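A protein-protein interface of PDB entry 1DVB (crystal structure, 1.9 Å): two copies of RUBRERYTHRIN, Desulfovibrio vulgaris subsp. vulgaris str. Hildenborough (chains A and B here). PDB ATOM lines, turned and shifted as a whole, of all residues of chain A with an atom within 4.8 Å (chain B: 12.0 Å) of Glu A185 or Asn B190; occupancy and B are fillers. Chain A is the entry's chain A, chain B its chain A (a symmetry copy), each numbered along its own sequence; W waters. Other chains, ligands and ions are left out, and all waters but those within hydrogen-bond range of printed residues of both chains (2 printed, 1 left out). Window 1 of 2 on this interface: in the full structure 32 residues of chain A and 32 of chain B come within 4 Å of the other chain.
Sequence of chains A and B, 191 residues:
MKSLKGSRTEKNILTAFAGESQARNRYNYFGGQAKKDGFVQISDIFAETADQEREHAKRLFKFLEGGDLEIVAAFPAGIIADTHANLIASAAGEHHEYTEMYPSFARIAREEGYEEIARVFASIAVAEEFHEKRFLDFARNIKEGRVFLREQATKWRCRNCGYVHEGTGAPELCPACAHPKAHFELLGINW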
ATOM      1  N   GLN A  41      -3.548 -32.864  16.300  1.00  0.00           N
ATOM      2  CA  GLN A  41      -4.256 -31.705  16.824  1.00  0.00           C
ATOM      3  C   GLN A  41      -3.346 -30.608  17.361  1.00  0.00           C
ATOM      4  O   GLN A  41      -3.574 -29.413  17.200  1.00  0.00           O
ATOM      5  CB  GLN A  41      -5.189 -32.181  17.965  1.00  0.00           C
ATOM      6  CG  GLN A  41      -5.878 -30.976  18.591  1.00  0.00           C
ATOM      7  CD  GLN A  41      -6.673 -31.286  19.852  1.00  0.00           C
ATOM      8  OE1 GLN A  41      -6.390 -32.235  20.545  1.00  0.00           O
ATOM      9  NE2 GLN A  41      -7.669 -30.498  20.162  1.00  0.00           N
ATOM     10  N   LYS A 155     -16.115 -39.141  23.668  1.00  0.00           N
ATOM     11  CA  LYS A 155     -16.007 -39.311  22.218  1.00  0.00           C
ATOM     12  C   LYS A 155     -14.870 -38.444  21.646  1.00  0.00           C
ATOM     13  O   LYS A 155     -14.649 -37.282  21.972  1.00  0.00           O
ATOM     14  CB  LYS A 155     -17.323 -39.023  21.519  1.00  0.00           C
ATOM     15  CG  LYS A 155     -18.170 -37.900  22.045  1.00  0.00           C
ATOM     16  CD  LYS A 155     -19.465 -38.389  22.696  1.00  0.00           C
ATOM     17  CE  LYS A 155     -20.554 -38.678  21.674  1.00  0.00           C
ATOM     18  NZ  LYS A 155     -21.954 -38.532  22.166  1.00  0.00           N
ATOM     19  N   TRP A 156     -14.195 -39.169  20.760  1.00  0.00           N
ATOM     20  CA  TRP A 156     -13.044 -38.835  19.950  1.00  0.00           C
ATOM     21  C   TRP A 156     -13.403 -38.540  18.487  1.00  0.00           C
ATOM     22  O   TRP A 156     -14.143 -39.322  17.881  1.00  0.00           O
ATOM     23  CB  TRP A 156     -12.023 -39.986  19.982  1.00  0.00           C
ATOM     24  CG  TRP A 156     -11.680 -40.355  21.394  1.00  0.00           C
ATOM     25  CD1 TRP A 156     -12.294 -41.279  22.225  1.00  0.00           C
ATOM     26  CD2 TRP A 156     -10.598 -39.766  22.132  1.00  0.00           C
ATOM     27  NE1 TRP A 156     -11.651 -41.299  23.442  1.00  0.00           N
ATOM     28  CE2 TRP A 156     -10.617 -40.387  23.413  1.00  0.00           C
ATOM     29  CE3 TRP A 156      -9.652 -38.787  21.799  1.00  0.00           C
ATOM     30  CZ2 TRP A 156      -9.676 -40.026  24.383  1.00  0.00           C
ATOM     31  CZ3 TRP A 156      -8.716 -38.426  22.754  1.00  0.00           C
ATOM     32  CH2 TRP A 156      -8.758 -39.055  24.010  1.00  0.00           C
ATOM     33  N   ARG A 157     -12.899 -37.444  17.914  1.00  0.00           N
ATOM     34  CA  ARG A 157     -13.159 -37.148  16.506  1.00  0.00           C
ATOM     35  C   ARG A 157     -11.835 -37.224  15.723  1.00  0.00           C
ATOM     36  O   ARG A 157     -10.757 -36.792  16.105  1.00  0.00           O
ATOM     37  CB  ARG A 157     -13.886 -35.808  16.371  1.00  0.00           C
ATOM     38  CG  ARG A 157     -14.496 -35.541  14.994  1.00  0.00           C
ATOM     39  CD  ARG A 157     -14.873 -34.080  14.817  1.00  0.00           C
ATOM     40  NE  ARG A 157     -13.683 -33.207  14.846  1.00  0.00           N
ATOM     41  CZ  ARG A 157     -13.466 -32.219  13.989  1.00  0.00           C
ATOM     42  NH1 ARG A 157     -14.332 -31.939  13.015  1.00  0.00           N
ATOM     43  NH2 ARG A 157     -12.389 -31.450  14.039  1.00  0.00           N
ATOM     44  N   ARG A 159      -9.757 -35.912  12.898  1.00  0.00           N
ATOM     45  CA  ARG A 159      -9.581 -34.596  12.294  1.00  0.00           C
ATOM     46  C   ARG A 159      -9.569 -34.751  10.777  1.00  0.00           C
ATOM     47  O   ARG A 159      -9.959 -33.835  10.071  1.00  0.00           O
ATOM     48  CB  ARG A 159      -8.306 -33.939  12.811  1.00  0.00           C
ATOM     49  CG  ARG A 159      -8.488 -33.683  14.305  1.00  0.00           C
ATOM     50  CD  ARG A 159      -7.544 -32.675  14.908  1.00  0.00           C
ATOM     51  NE  ARG A 159      -8.110 -31.293  14.686  1.00  0.00           N
ATOM     52  CZ  ARG A 159      -7.244 -30.604  13.950  1.00  0.00           C
ATOM     53  NH1 ARG A 159      -6.166 -31.344  13.653  1.00  0.00           N
ATOM     54  NH2 ARG A 159      -7.400 -29.378  13.558  1.00  0.00           N
ATOM     55  N   HIS A 183      -4.519 -38.645  14.342  1.00  0.00           N
ATOM     56  CA  HIS A 183      -5.483 -37.694  13.804  1.00  0.00           C
ATOM     57  C   HIS A 183      -6.659 -37.397  14.724  1.00  0.00           C
ATOM     58  O   HIS A 183      -7.447 -36.472  14.474  1.00  0.00           O
ATOM     59  CB  HIS A 183      -5.983 -38.263  12.448  1.00  0.00           C
ATOM     60  CG  HIS A 183      -4.873 -38.147  11.444  1.00  0.00           C
ATOM     61  ND1 HIS A 183      -4.771 -37.053  10.610  1.00  0.00           N
ATOM     62  CD2 HIS A 183      -3.832 -38.957  11.143  1.00  0.00           C
ATOM     63  CE1 HIS A 183      -3.703 -37.205   9.825  1.00  0.00           C
ATOM     64  NE2 HIS A 183      -3.104 -38.351  10.123  1.00  0.00           N
ATOM     65  N   PHE A 184      -6.763 -38.189  15.783  1.00  0.00           N
ATOM     66  CA  PHE A 184      -7.921 -38.031  16.690  1.00  0.00           C
ATOM     67  C   PHE A 184      -7.783 -36.982  17.769  1.00  0.00           C
ATOM     68  O   PHE A 184      -6.676 -36.716  18.278  1.00  0.00           O
ATOM     69  CB  PHE A 184      -8.198 -39.408  17.356  1.00  0.00           C
ATOM     70  CG  PHE A 184      -8.998 -40.271  16.371  1.00  0.00           C
ATOM     71  CD1 PHE A 184     -10.390 -40.143  16.325  1.00  0.00           C
ATOM     72  CD2 PHE A 184      -8.315 -41.161  15.548  1.00  0.00           C
ATOM     73  CE1 PHE A 184     -11.120 -40.910  15.441  1.00  0.00           C
ATOM     74  CE2 PHE A 184      -9.048 -41.938  14.646  1.00  0.00           C
ATOM     75  CZ  PHE A 184     -10.427 -41.803  14.613  1.00  0.00           C
ATOM     76  N   GLU A 185      -8.922 -36.402  18.115  1.00  0.00           N
ATOM     77  CA  GLU A 185      -9.001 -35.401  19.158  1.00  0.00           C
ATOM     78  C   GLU A 185     -10.236 -35.589  20.040  1.00  0.00           C
ATOM     79  O   GLU A 185     -11.109 -36.374  19.693  1.00  0.00           O
ATOM     80  CB  GLU A 185      -9.121 -33.982  18.598  1.00  0.00           C
ATOM     81  CG  GLU A 185     -10.440 -33.737  17.923  1.00  0.00           C
ATOM     82  CD  GLU A 185     -10.567 -32.418  17.209  1.00  0.00           C
ATOM     83  OE1 GLU A 185      -9.557 -31.699  17.169  1.00  0.00           O
ATOM     84  OE2 GLU A 185     -11.669 -32.091  16.684  1.00  0.00           O
ATOM     85  N   LEU A 186     -10.351 -34.882  21.161  1.00  0.00           N
ATOM     86  CA  LEU A 186     -11.585 -34.983  21.956  1.00  0.00           C
ATOM     87  C   LEU A 186     -12.687 -34.344  21.154  1.00  0.00           C
ATOM     88  O   LEU A 186     -12.487 -33.251  20.619  1.00  0.00           O
ATOM     89  CB  LEU A 186     -11.456 -34.321  23.339  1.00  0.00           C
ATOM     90  CG  LEU A 186     -10.792 -35.281  24.341  1.00  0.00           C
ATOM     91  CD1 LEU A 186     -10.340 -34.551  25.594  1.00  0.00           C
ATOM     92  CD2 LEU A 186     -11.739 -36.419  24.673  1.00  0.00           C
ATOM     93  N   LEU A 187     -13.863 -34.931  21.018  1.00  0.00           N
ATOM     94  CA  LEU A 187     -14.798 -34.129  20.239  1.00  0.00           C
ATOM     95  C   LEU A 187     -15.235 -32.867  20.963  1.00  0.00           C
ATOM     96  O   LEU A 187     -15.603 -33.064  22.135  1.00  0.00           O
ATOM     97  CB  LEU A 187     -16.072 -34.926  19.930  1.00  0.00           C
ATOM     98  CG  LEU A 187     -17.086 -34.151  19.066  1.00  0.00           C
ATOM     99  CD1 LEU A 187     -17.570 -34.987  17.903  1.00  0.00           C
ATOM    100  CD2 LEU A 187     -18.258 -33.677  19.909  1.00  0.00           C
ATOM    101  N   GLY A 188     -15.235 -31.675  20.364  1.00  0.00           N
ATOM    102  CA  GLY A 188     -15.690 -30.447  20.979  1.00  0.00           C
ATOM    103  C   GLY A 188     -16.749 -29.663  20.243  1.00  0.00           C
ATOM    104  O   GLY A 188     -16.755 -29.600  19.023  1.00  0.00           O
ATOM    105  N   GLN B  41     -16.588 -18.132  11.620  1.00  0.00           N
ATOM    106  CA  GLN B  41     -16.477 -19.490  12.132  1.00  0.00           C
ATOM    107  C   GLN B  41     -17.220 -20.531  11.305  1.00  0.00           C
ATOM    108  O   GLN B  41     -16.773 -21.654  11.088  1.00  0.00           O
ATOM    109  CB  GLN B  41     -17.034 -19.512  13.577  1.00  0.00           C
ATOM    110  CG  GLN B  41     -17.011 -20.939  14.107  1.00  0.00           C
ATOM    111  CD  GLN B  41     -17.713 -21.129  15.445  1.00  0.00           C
ATOM    112  OE1 GLN B  41     -18.596 -20.380  15.792  1.00  0.00           O
ATOM    113  NE2 GLN B  41     -17.333 -22.122  16.205  1.00  0.00           N
ATOM    114  N   ASP B  44     -15.216 -21.263   8.105  1.00  0.00           N
ATOM    115  CA  ASP B  44     -14.239 -22.330   8.323  1.00  0.00           C
ATOM    116  C   ASP B  44     -14.812 -23.710   8.543  1.00  0.00           C
ATOM    117  O   ASP B  44     -14.154 -24.733   8.252  1.00  0.00           O
ATOM    118  CB  ASP B  44     -13.386 -21.926   9.543  1.00  0.00           C
ATOM    119  CG  ASP B  44     -12.497 -20.738   9.195  1.00  0.00           C
ATOM    120  OD1 ASP B  44     -12.444 -20.254   8.039  1.00  0.00           O
ATOM    121  OD2 ASP B  44     -11.805 -20.220  10.090  1.00  0.00           O
ATOM    122  N   ILE B  45     -16.046 -23.854   9.053  1.00  0.00           N
ATOM    123  CA  ILE B  45     -16.513 -25.261   9.212  1.00  0.00           C
ATOM    124  C   ILE B  45     -16.960 -25.843   7.872  1.00  0.00           C
ATOM    125  O   ILE B  45     -16.721 -27.006   7.589  1.00  0.00           O
ATOM    126  CB  ILE B  45     -17.577 -25.281  10.325  1.00  0.00           C
ATOM    127  CG1 ILE B  45     -16.924 -25.530  11.726  1.00  0.00           C
ATOM    128  CG2 ILE B  45     -18.739 -26.243  10.127  1.00  0.00           C
ATOM    129  CD1 ILE B  45     -17.157 -24.247  12.510  1.00  0.00           C
ATOM    130  N   GLU B  48     -13.842 -26.893   6.504  1.00  0.00           N
ATOM    131  CA  GLU B  48     -13.376 -28.144   7.063  1.00  0.00           C
ATOM    132  C   GLU B  48     -14.161 -29.362   6.570  1.00  0.00           C
ATOM    133  O   GLU B  48     -13.638 -30.439   6.241  1.00  0.00           O
ATOM    134  CB  GLU B  48     -13.521 -28.142   8.597  1.00  0.00           C
ATOM    135  CG  GLU B  48     -12.879 -29.446   9.173  1.00  0.00           C
ATOM    136  CD  GLU B  48     -13.370 -29.495  10.640  1.00  0.00           C
ATOM    137  OE1 GLU B  48     -14.512 -29.970  10.876  1.00  0.00           O
ATOM    138  OE2 GLU B  48     -12.629 -29.049  11.546  1.00  0.00           O
ATOM    139  N   THR B  49     -15.491 -29.180   6.525  1.00  0.00           N
ATOM    140  CA  THR B  49     -16.339 -30.280   6.033  1.00  0.00           C
ATOM    141  C   THR B  49     -15.956 -30.641   4.606  1.00  0.00           C
ATOM    142  O   THR B  49     -15.823 -31.859   4.299  1.00  0.00           O
ATOM    143  CB  THR B  49     -17.817 -29.890   6.155  1.00  0.00           C
ATOM    144  OG1 THR B  49     -18.082 -29.473   7.517  1.00  0.00           O
ATOM    145  CG2 THR B  49     -18.705 -31.089   5.897  1.00  0.00           C
ATOM    146  N   GLN B  52     -13.017 -32.814   4.738  1.00  0.00           N
ATOM    147  CA  GLN B  52     -13.347 -34.200   5.180  1.00  0.00           C
ATOM    148  C   GLN B  52     -14.083 -34.940   4.074  1.00  0.00           C
ATOM    149  O   GLN B  52     -13.904 -36.142   3.956  1.00  0.00           O
ATOM    150  CB  GLN B  52     -14.133 -34.126   6.486  1.00  0.00           C
ATOM    151  CG  GLN B  52     -13.159 -33.614   7.577  1.00  0.00           C
ATOM    152  CD  GLN B  52     -13.775 -33.409   8.960  1.00  0.00           C
ATOM    153  OE1 GLN B  52     -14.998 -33.182   9.091  1.00  0.00           O
ATOM    154  NE2 GLN B  52     -12.929 -33.486   9.985  1.00  0.00           N
ATOM    155  N   ALA B 127     -19.801 -40.142  10.352  1.00  0.00           N
ATOM    156  CA  ALA B 127     -19.270 -38.802  10.127  1.00  0.00           C
ATOM    157  C   ALA B 127     -20.343 -37.897   9.568  1.00  0.00           C
ATOM    158  O   ALA B 127     -20.452 -36.740   9.959  1.00  0.00           O
ATOM    159  CB  ALA B 127     -18.078 -38.806   9.162  1.00  0.00           C
ATOM    160  N   PHE B 130     -22.548 -36.408  12.312  1.00  0.00           N
ATOM    161  CA  PHE B 130     -22.047 -35.251  13.065  1.00  0.00           C
ATOM    162  C   PHE B 130     -22.052 -34.006  12.193  1.00  0.00           C
ATOM    163  O   PHE B 130     -22.331 -32.861  12.653  1.00  0.00           O
ATOM    164  CB  PHE B 130     -20.685 -35.667  13.658  1.00  0.00           C
ATOM    165  CG  PHE B 130     -20.059 -34.456  14.347  1.00  0.00           C
ATOM    166  CD1 PHE B 130     -20.769 -33.753  15.312  1.00  0.00           C
ATOM    167  CD2 PHE B 130     -18.787 -34.011  14.042  1.00  0.00           C
ATOM    168  CE1 PHE B 130     -20.217 -32.637  15.939  1.00  0.00           C
ATOM    169  CE2 PHE B 130     -18.222 -32.898  14.656  1.00  0.00           C
ATOM    170  CZ  PHE B 130     -18.936 -32.205  15.609  1.00  0.00           C
ATOM    171  N   HIS B 131     -21.760 -34.219  10.876  1.00  0.00           N
ATOM    172  CA  HIS B 131     -21.765 -33.050  10.005  1.00  0.00           C
ATOM    173  C   HIS B 131     -23.141 -32.418  10.034  1.00  0.00           C
ATOM    174  O   HIS B 131     -23.342 -31.209  10.159  1.00  0.00           O
ATOM    175  CB  HIS B 131     -21.386 -33.332   8.522  1.00  0.00           C
ATOM    176  CG  HIS B 131     -20.022 -33.839   8.158  1.00  0.00           C
ATOM    177  ND1 HIS B 131     -19.717 -34.621   7.045  1.00  0.00           N
ATOM    178  CD2 HIS B 131     -18.843 -33.652   8.804  1.00  0.00           C
ATOM    179  CE1 HIS B 131     -18.403 -34.862   7.086  1.00  0.00           C
ATOM    180  NE2 HIS B 131     -17.832 -34.288   8.135  1.00  0.00           N
ATOM    181  N   ARG B 134     -23.841 -30.481  13.283  1.00  0.00           N
ATOM    182  CA  ARG B 134     -23.150 -29.194  13.268  1.00  0.00           C
ATOM    183  C   ARG B 134     -23.920 -28.164  12.475  1.00  0.00           C
ATOM    184  O   ARG B 134     -24.197 -27.014  12.837  1.00  0.00           O
ATOM    185  CB  ARG B 134     -21.754 -29.411  12.674  1.00  0.00           C
ATOM    186  CG  ARG B 134     -20.636 -29.344  13.680  1.00  0.00           C
ATOM    187  CD  ARG B 134     -19.283 -29.149  13.078  1.00  0.00           C
ATOM    188  NE  ARG B 134     -19.020 -29.682  11.730  1.00  0.00           N
ATOM    189  CZ  ARG B 134     -17.710 -29.804  11.462  1.00  0.00           C
ATOM    190  NH1 ARG B 134     -16.855 -29.442  12.421  1.00  0.00           N
ATOM    191  NH2 ARG B 134     -17.179 -30.246  10.352  1.00  0.00           N
ATOM    192  N   ARG B 157     -13.872 -15.767  21.523  1.00  0.00           N
ATOM    193  CA  ARG B 157     -12.505 -15.693  21.009  1.00  0.00           C
ATOM    194  C   ARG B 157     -12.540 -15.187  19.555  1.00  0.00           C
ATOM    195  O   ARG B 157     -13.347 -15.528  18.702  1.00  0.00           O
ATOM    196  CB  ARG B 157     -11.799 -17.041  21.182  1.00  0.00           C
ATOM    197  CG  ARG B 157     -10.284 -17.005  20.986  1.00  0.00           C
ATOM    198  CD  ARG B 157      -9.704 -18.399  20.811  1.00  0.00           C
ATOM    199  NE  ARG B 157     -10.200 -19.039  19.577  1.00  0.00           N
ATOM    200  CZ  ARG B 157      -9.430 -19.698  18.722  1.00  0.00           C
ATOM    201  NH1 ARG B 157      -8.119 -19.830  18.923  1.00  0.00           N
ATOM    202  NH2 ARG B 157      -9.902 -20.266  17.623  1.00  0.00           N
ATOM    203  N   ARG B 159     -11.020 -15.298  16.135  1.00  0.00           N
ATOM    204  CA  ARG B 159     -10.389 -16.345  15.338  1.00  0.00           C
ATOM    205  C   ARG B 159      -9.144 -15.770  14.673  1.00  0.00           C
ATOM    206  O   ARG B 159      -8.200 -16.501  14.419  1.00  0.00           O
ATOM    207  CB  ARG B 159     -11.374 -16.905  14.319  1.00  0.00           C
ATOM    208  CG  ARG B 159     -12.497 -17.596  15.089  1.00  0.00           C
ATOM    209  CD  ARG B 159     -13.328 -18.567  14.289  1.00  0.00           C
ATOM    210  NE  ARG B 159     -12.626 -19.903  14.275  1.00  0.00           N
ATOM    211  CZ  ARG B 159     -12.341 -20.208  13.013  1.00  0.00           C
ATOM    212  NH1 ARG B 159     -12.765 -19.250  12.177  1.00  0.00           N
ATOM    213  NH2 ARG B 159     -11.732 -21.283  12.619  1.00  0.00           N
ATOM    214  N   GLU B 185     -15.921 -16.165  17.974  1.00  0.00           N
ATOM    215  CA  GLU B 185     -16.596 -17.418  18.241  1.00  0.00           C
ATOM    216  C   GLU B 185     -16.733 -17.688  19.740  1.00  0.00           C
ATOM    217  O   GLU B 185     -16.118 -16.989  20.535  1.00  0.00           O
ATOM    218  CB  GLU B 185     -15.833 -18.623  17.685  1.00  0.00           C
ATOM    219  CG  GLU B 185     -14.546 -18.878  18.415  1.00  0.00           C
ATOM    220  CD  GLU B 185     -13.666 -19.946  17.823  1.00  0.00           C
ATOM    221  OE1 GLU B 185     -14.036 -20.451  16.752  1.00  0.00           O
ATOM    222  OE2 GLU B 185     -12.603 -20.286  18.416  1.00  0.00           O
ATOM    223  N   LEU B 186     -17.503 -18.690  20.154  1.00  0.00           N
ATOM    224  CA  LEU B 186     -17.553 -19.018  21.588  1.00  0.00           C
ATOM    225  C   LEU B 186     -16.206 -19.576  21.966  1.00  0.00           C
ATOM    226  O   LEU B 186     -15.683 -20.427  21.244  1.00  0.00           O
ATOM    227  CB  LEU B 186     -18.676 -20.012  21.931  1.00  0.00           C
ATOM    228  CG  LEU B 186     -20.017 -19.278  22.104  1.00  0.00           C
ATOM    229  CD1 LEU B 186     -21.186 -20.247  22.096  1.00  0.00           C
ATOM    230  CD2 LEU B 186     -19.993 -18.448  23.374  1.00  0.00           C
ATOM    231  N   LEU B 187     -15.582 -19.172  23.059  1.00  0.00           N
ATOM    232  CA  LEU B 187     -14.315 -19.863  23.262  1.00  0.00           C
ATOM    233  C   LEU B 187     -14.494 -21.332  23.608  1.00  0.00           C
ATOM    234  O   LEU B 187     -15.323 -21.534  24.514  1.00  0.00           O
ATOM    235  CB  LEU B 187     -13.527 -19.229  24.415  1.00  0.00           C
ATOM    236  CG  LEU B 187     -12.152 -19.883  24.653  1.00  0.00           C
ATOM    237  CD1 LEU B 187     -11.059 -18.845  24.759  1.00  0.00           C
ATOM    238  CD2 LEU B 187     -12.181 -20.758  25.895  1.00  0.00           C
ATOM    239  N   GLY B 188     -13.798 -22.291  22.997  1.00  0.00           N
ATOM    240  CA  GLY B 188     -13.882 -23.699  23.319  1.00  0.00           C
ATOM    241  C   GLY B 188     -12.590 -24.406  23.650  1.00  0.00           C
ATOM    242  O   GLY B 188     -11.550 -24.123  23.075  1.00  0.00           O
ATOM    243  N   ILE B 189     -12.660 -25.337  24.580  1.00  0.00           N
ATOM    244  CA  ILE B 189     -11.587 -26.162  25.064  1.00  0.00           C
ATOM    245  C   ILE B 189     -11.883 -27.614  24.686  1.00  0.00           C
ATOM    246  O   ILE B 189     -13.030 -27.968  25.004  1.00  0.00           O
ATOM    247  CB  ILE B 189     -11.427 -26.137  26.586  1.00  0.00           C
ATOM    248  CG1 ILE B 189     -11.541 -24.742  27.212  1.00  0.00           C
ATOM    249  CG2 ILE B 189     -10.122 -26.785  27.014  1.00  0.00           C
ATOM    250  CD1 ILE B 189     -10.689 -23.677  26.583  1.00  0.00           C
ATOM    251  N   ASN B 190     -10.959 -28.364  24.081  1.00  0.00           N
ATOM    252  CA  ASN B 190     -11.261 -29.755  23.710  1.00  0.00           C
ATOM    253  C   ASN B 190     -10.025 -30.659  23.754  1.00  0.00           C
ATOM    254  O   ASN B 190      -9.676 -31.371  22.804  1.00  0.00           O
ATOM    255  CB  ASN B 190     -11.957 -29.814  22.340  1.00  0.00           C
ATOM    256  CG  ASN B 190     -11.066 -29.614  21.135  1.00  0.00           C
ATOM    257  OD1 ASN B 190     -11.061 -30.496  20.273  1.00  0.00           O
ATOM    258  ND2 ASN B 190     -10.344 -28.493  21.085  1.00  0.00           N
ATOM    259  N   TRP B 191      -9.425 -30.598  24.933  1.00  0.00           N
ATOM    260  CA  TRP B 191      -8.234 -31.297  25.358  1.00  0.00           C
ATOM    261  C   TRP B 191      -8.166 -31.425  26.871  1.00  0.00           C
ATOM    262  O   TRP B 191      -7.491 -32.223  27.515  1.00  0.00           O
ATOM    263  CB  TRP B 191      -7.039 -30.509  24.826  1.00  0.00           C
ATOM    264  CG  TRP B 191      -7.087 -29.030  25.126  1.00  0.00           C
ATOM    265  CD1 TRP B 191      -6.674 -28.489  26.321  1.00  0.00           C
ATOM    266  CD2 TRP B 191      -7.522 -27.899  24.338  1.00  0.00           C
ATOM    267  NE1 TRP B 191      -6.826 -27.122  26.319  1.00  0.00           N
ATOM    268  CE2 TRP B 191      -7.347 -26.717  25.117  1.00  0.00           C
ATOM    269  CE3 TRP B 191      -8.053 -27.701  23.052  1.00  0.00           C
ATOM    270  CZ2 TRP B 191      -7.667 -25.428  24.670  1.00  0.00           C
ATOM    271  CZ3 TRP B 191      -8.369 -26.425  22.615  1.00  0.00           C
ATOM    272  CH2 TRP B 191      -8.186 -25.281  23.400  1.00  0.00           C
ATOM    273  OXT TRP B 191      -8.877 -30.617  27.584  1.00  0.00           O
HETATM  274  O   HOH W   1      -8.242 -33.326  22.460  1.00  0.00           O
HETATM  275  O   HOH W   2     -16.646 -33.163  11.729  1.00  0.00           O
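No residue of chain B comes within 4 Å of Trp A156.
Arg A157 touches just these residues of chain B: Glu B48 (2.9 Å), Gln B52 (3.7 Å), Phe B130 (3.6 Å) and Arg B134 (3.6 Å).
Of chain B, only Gln B52 (3.0 Å) comes within 4 Å of Arg A159.
Phe A184 touches none of the printed residues of chain B.
Glu A185 touches just one residue of chain B: Asn B190.
Of chain B, only Asn B190 (3.1 Å) and Trp B191 (3.9 Å) come within 4 Å of Leu A186.
No residue of chain B comes within 4 Å of Gly A188.
Of the printed residues of chain A, Glu B48 touches Arg A157.
Of the printed residues of chain A, Gln B52 touches Arg A157 and Arg A159.
Of the printed residues of chain A, Phe B130 touches Arg A157 and Leu A187.
Of the printed residues of chain A, Arg B134 touches Arg A157.
Arg B159 touches none of the printed residues of chain A.
Gly B188 touches none of the printed residues of chain A.
Asn B190 touches just these residues of chain A: Gln A41, Glu A185 and Leu A186.
The nearest residue of chain B that does not touch Glu A185 is Glu B48 (6.0 Å).
The nearest residue of chain A that does not touch Asn B190 is Gly A188 (4.02 Å).
7 positions are printed for both chains.
Of the 11 printed residues of chain A, 6 touch a printed residue of chain B.
Hydrophobic or aromatic side chains of chain A within 4 Å of the printed part of chain B: Leu A186 and Leu A187.
Hydrophobic or aromatic side chains of chain B that line the printed part of chain A: Phe B130.
Along chain B the printed residues that touch a printed residue of chain A span positions 48 to 191.
Among the printed residues, 10 pairs touch across the chains.
NH1 of Arg A157 touches NE2 of Gln B52 (3.7 Å).
Phe B130 touches Arg A157 (CE2 to CD, 3.6 Å).
Arg B134 touches Arg A157 (NH1 to NH1, 3.6 Å).
Asn B190 touches Glu A185.
Trp B191 touches Leu A186 (CA to CD1, 3.9 Å).
CZ of Phe B130 touches CD1 of Leu A187, at 3.9 Å.
OE2 of Glu A185 is in salt-bridge range of NH2 of Arg A157, 2.8 Å away.
N of Arg A159 lies within hydrogen-bond range of O of His A183 (2.9 Å).
NE of Arg A159 is in salt-bridge range of OE1 of Glu A185 (2.9 Å).
The side-chain carboxylate of Glu B48 is in salt-bridge range of the guanidinium group of Arg B134.
The side-chain hydroxyl of Thr B49 lies within hydrogen-bond range of the guanidinium group of Arg B134 (3.1 Å).
The side-chain amide oxygen of Gln B52 lies within hydrogen-bond range of a ring nitrogen (NE2) of His B131, 3.2 Å away.
The side-chain amide nitrogen (NE2) of Gln A41 is in hydrogen-bond range of the side-chain amide oxygen (OD1) of Asn B190 (3.4 Å).
The guanidinium group (NH1) of Arg A157 lies within salt-bridge range of the side-chain carboxylate (OE1) of Glu B48.
NE2 of Gln B52 lies within hydrogen-bond range of O of Arg A159 (3.0 Å).
The side-chain amide oxygen (OD1) of Asn B190 sits close to the backbone carbonyl oxygen (O) of Leu A186, 3.1 Å away.
Water W1 lies within hydrogen-bond range of the backbone carbonyl oxygen of Asn B190, the side-chain amide oxygen of Gln A41 and the backbone NH of Leu A186.
Water W2 lies within hydrogen-bond range of NH1 of Arg A157 (2.9 Å), OE1 of Gln B52 (3.1 Å) and NH2 of Arg B134 (3.3 Å).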
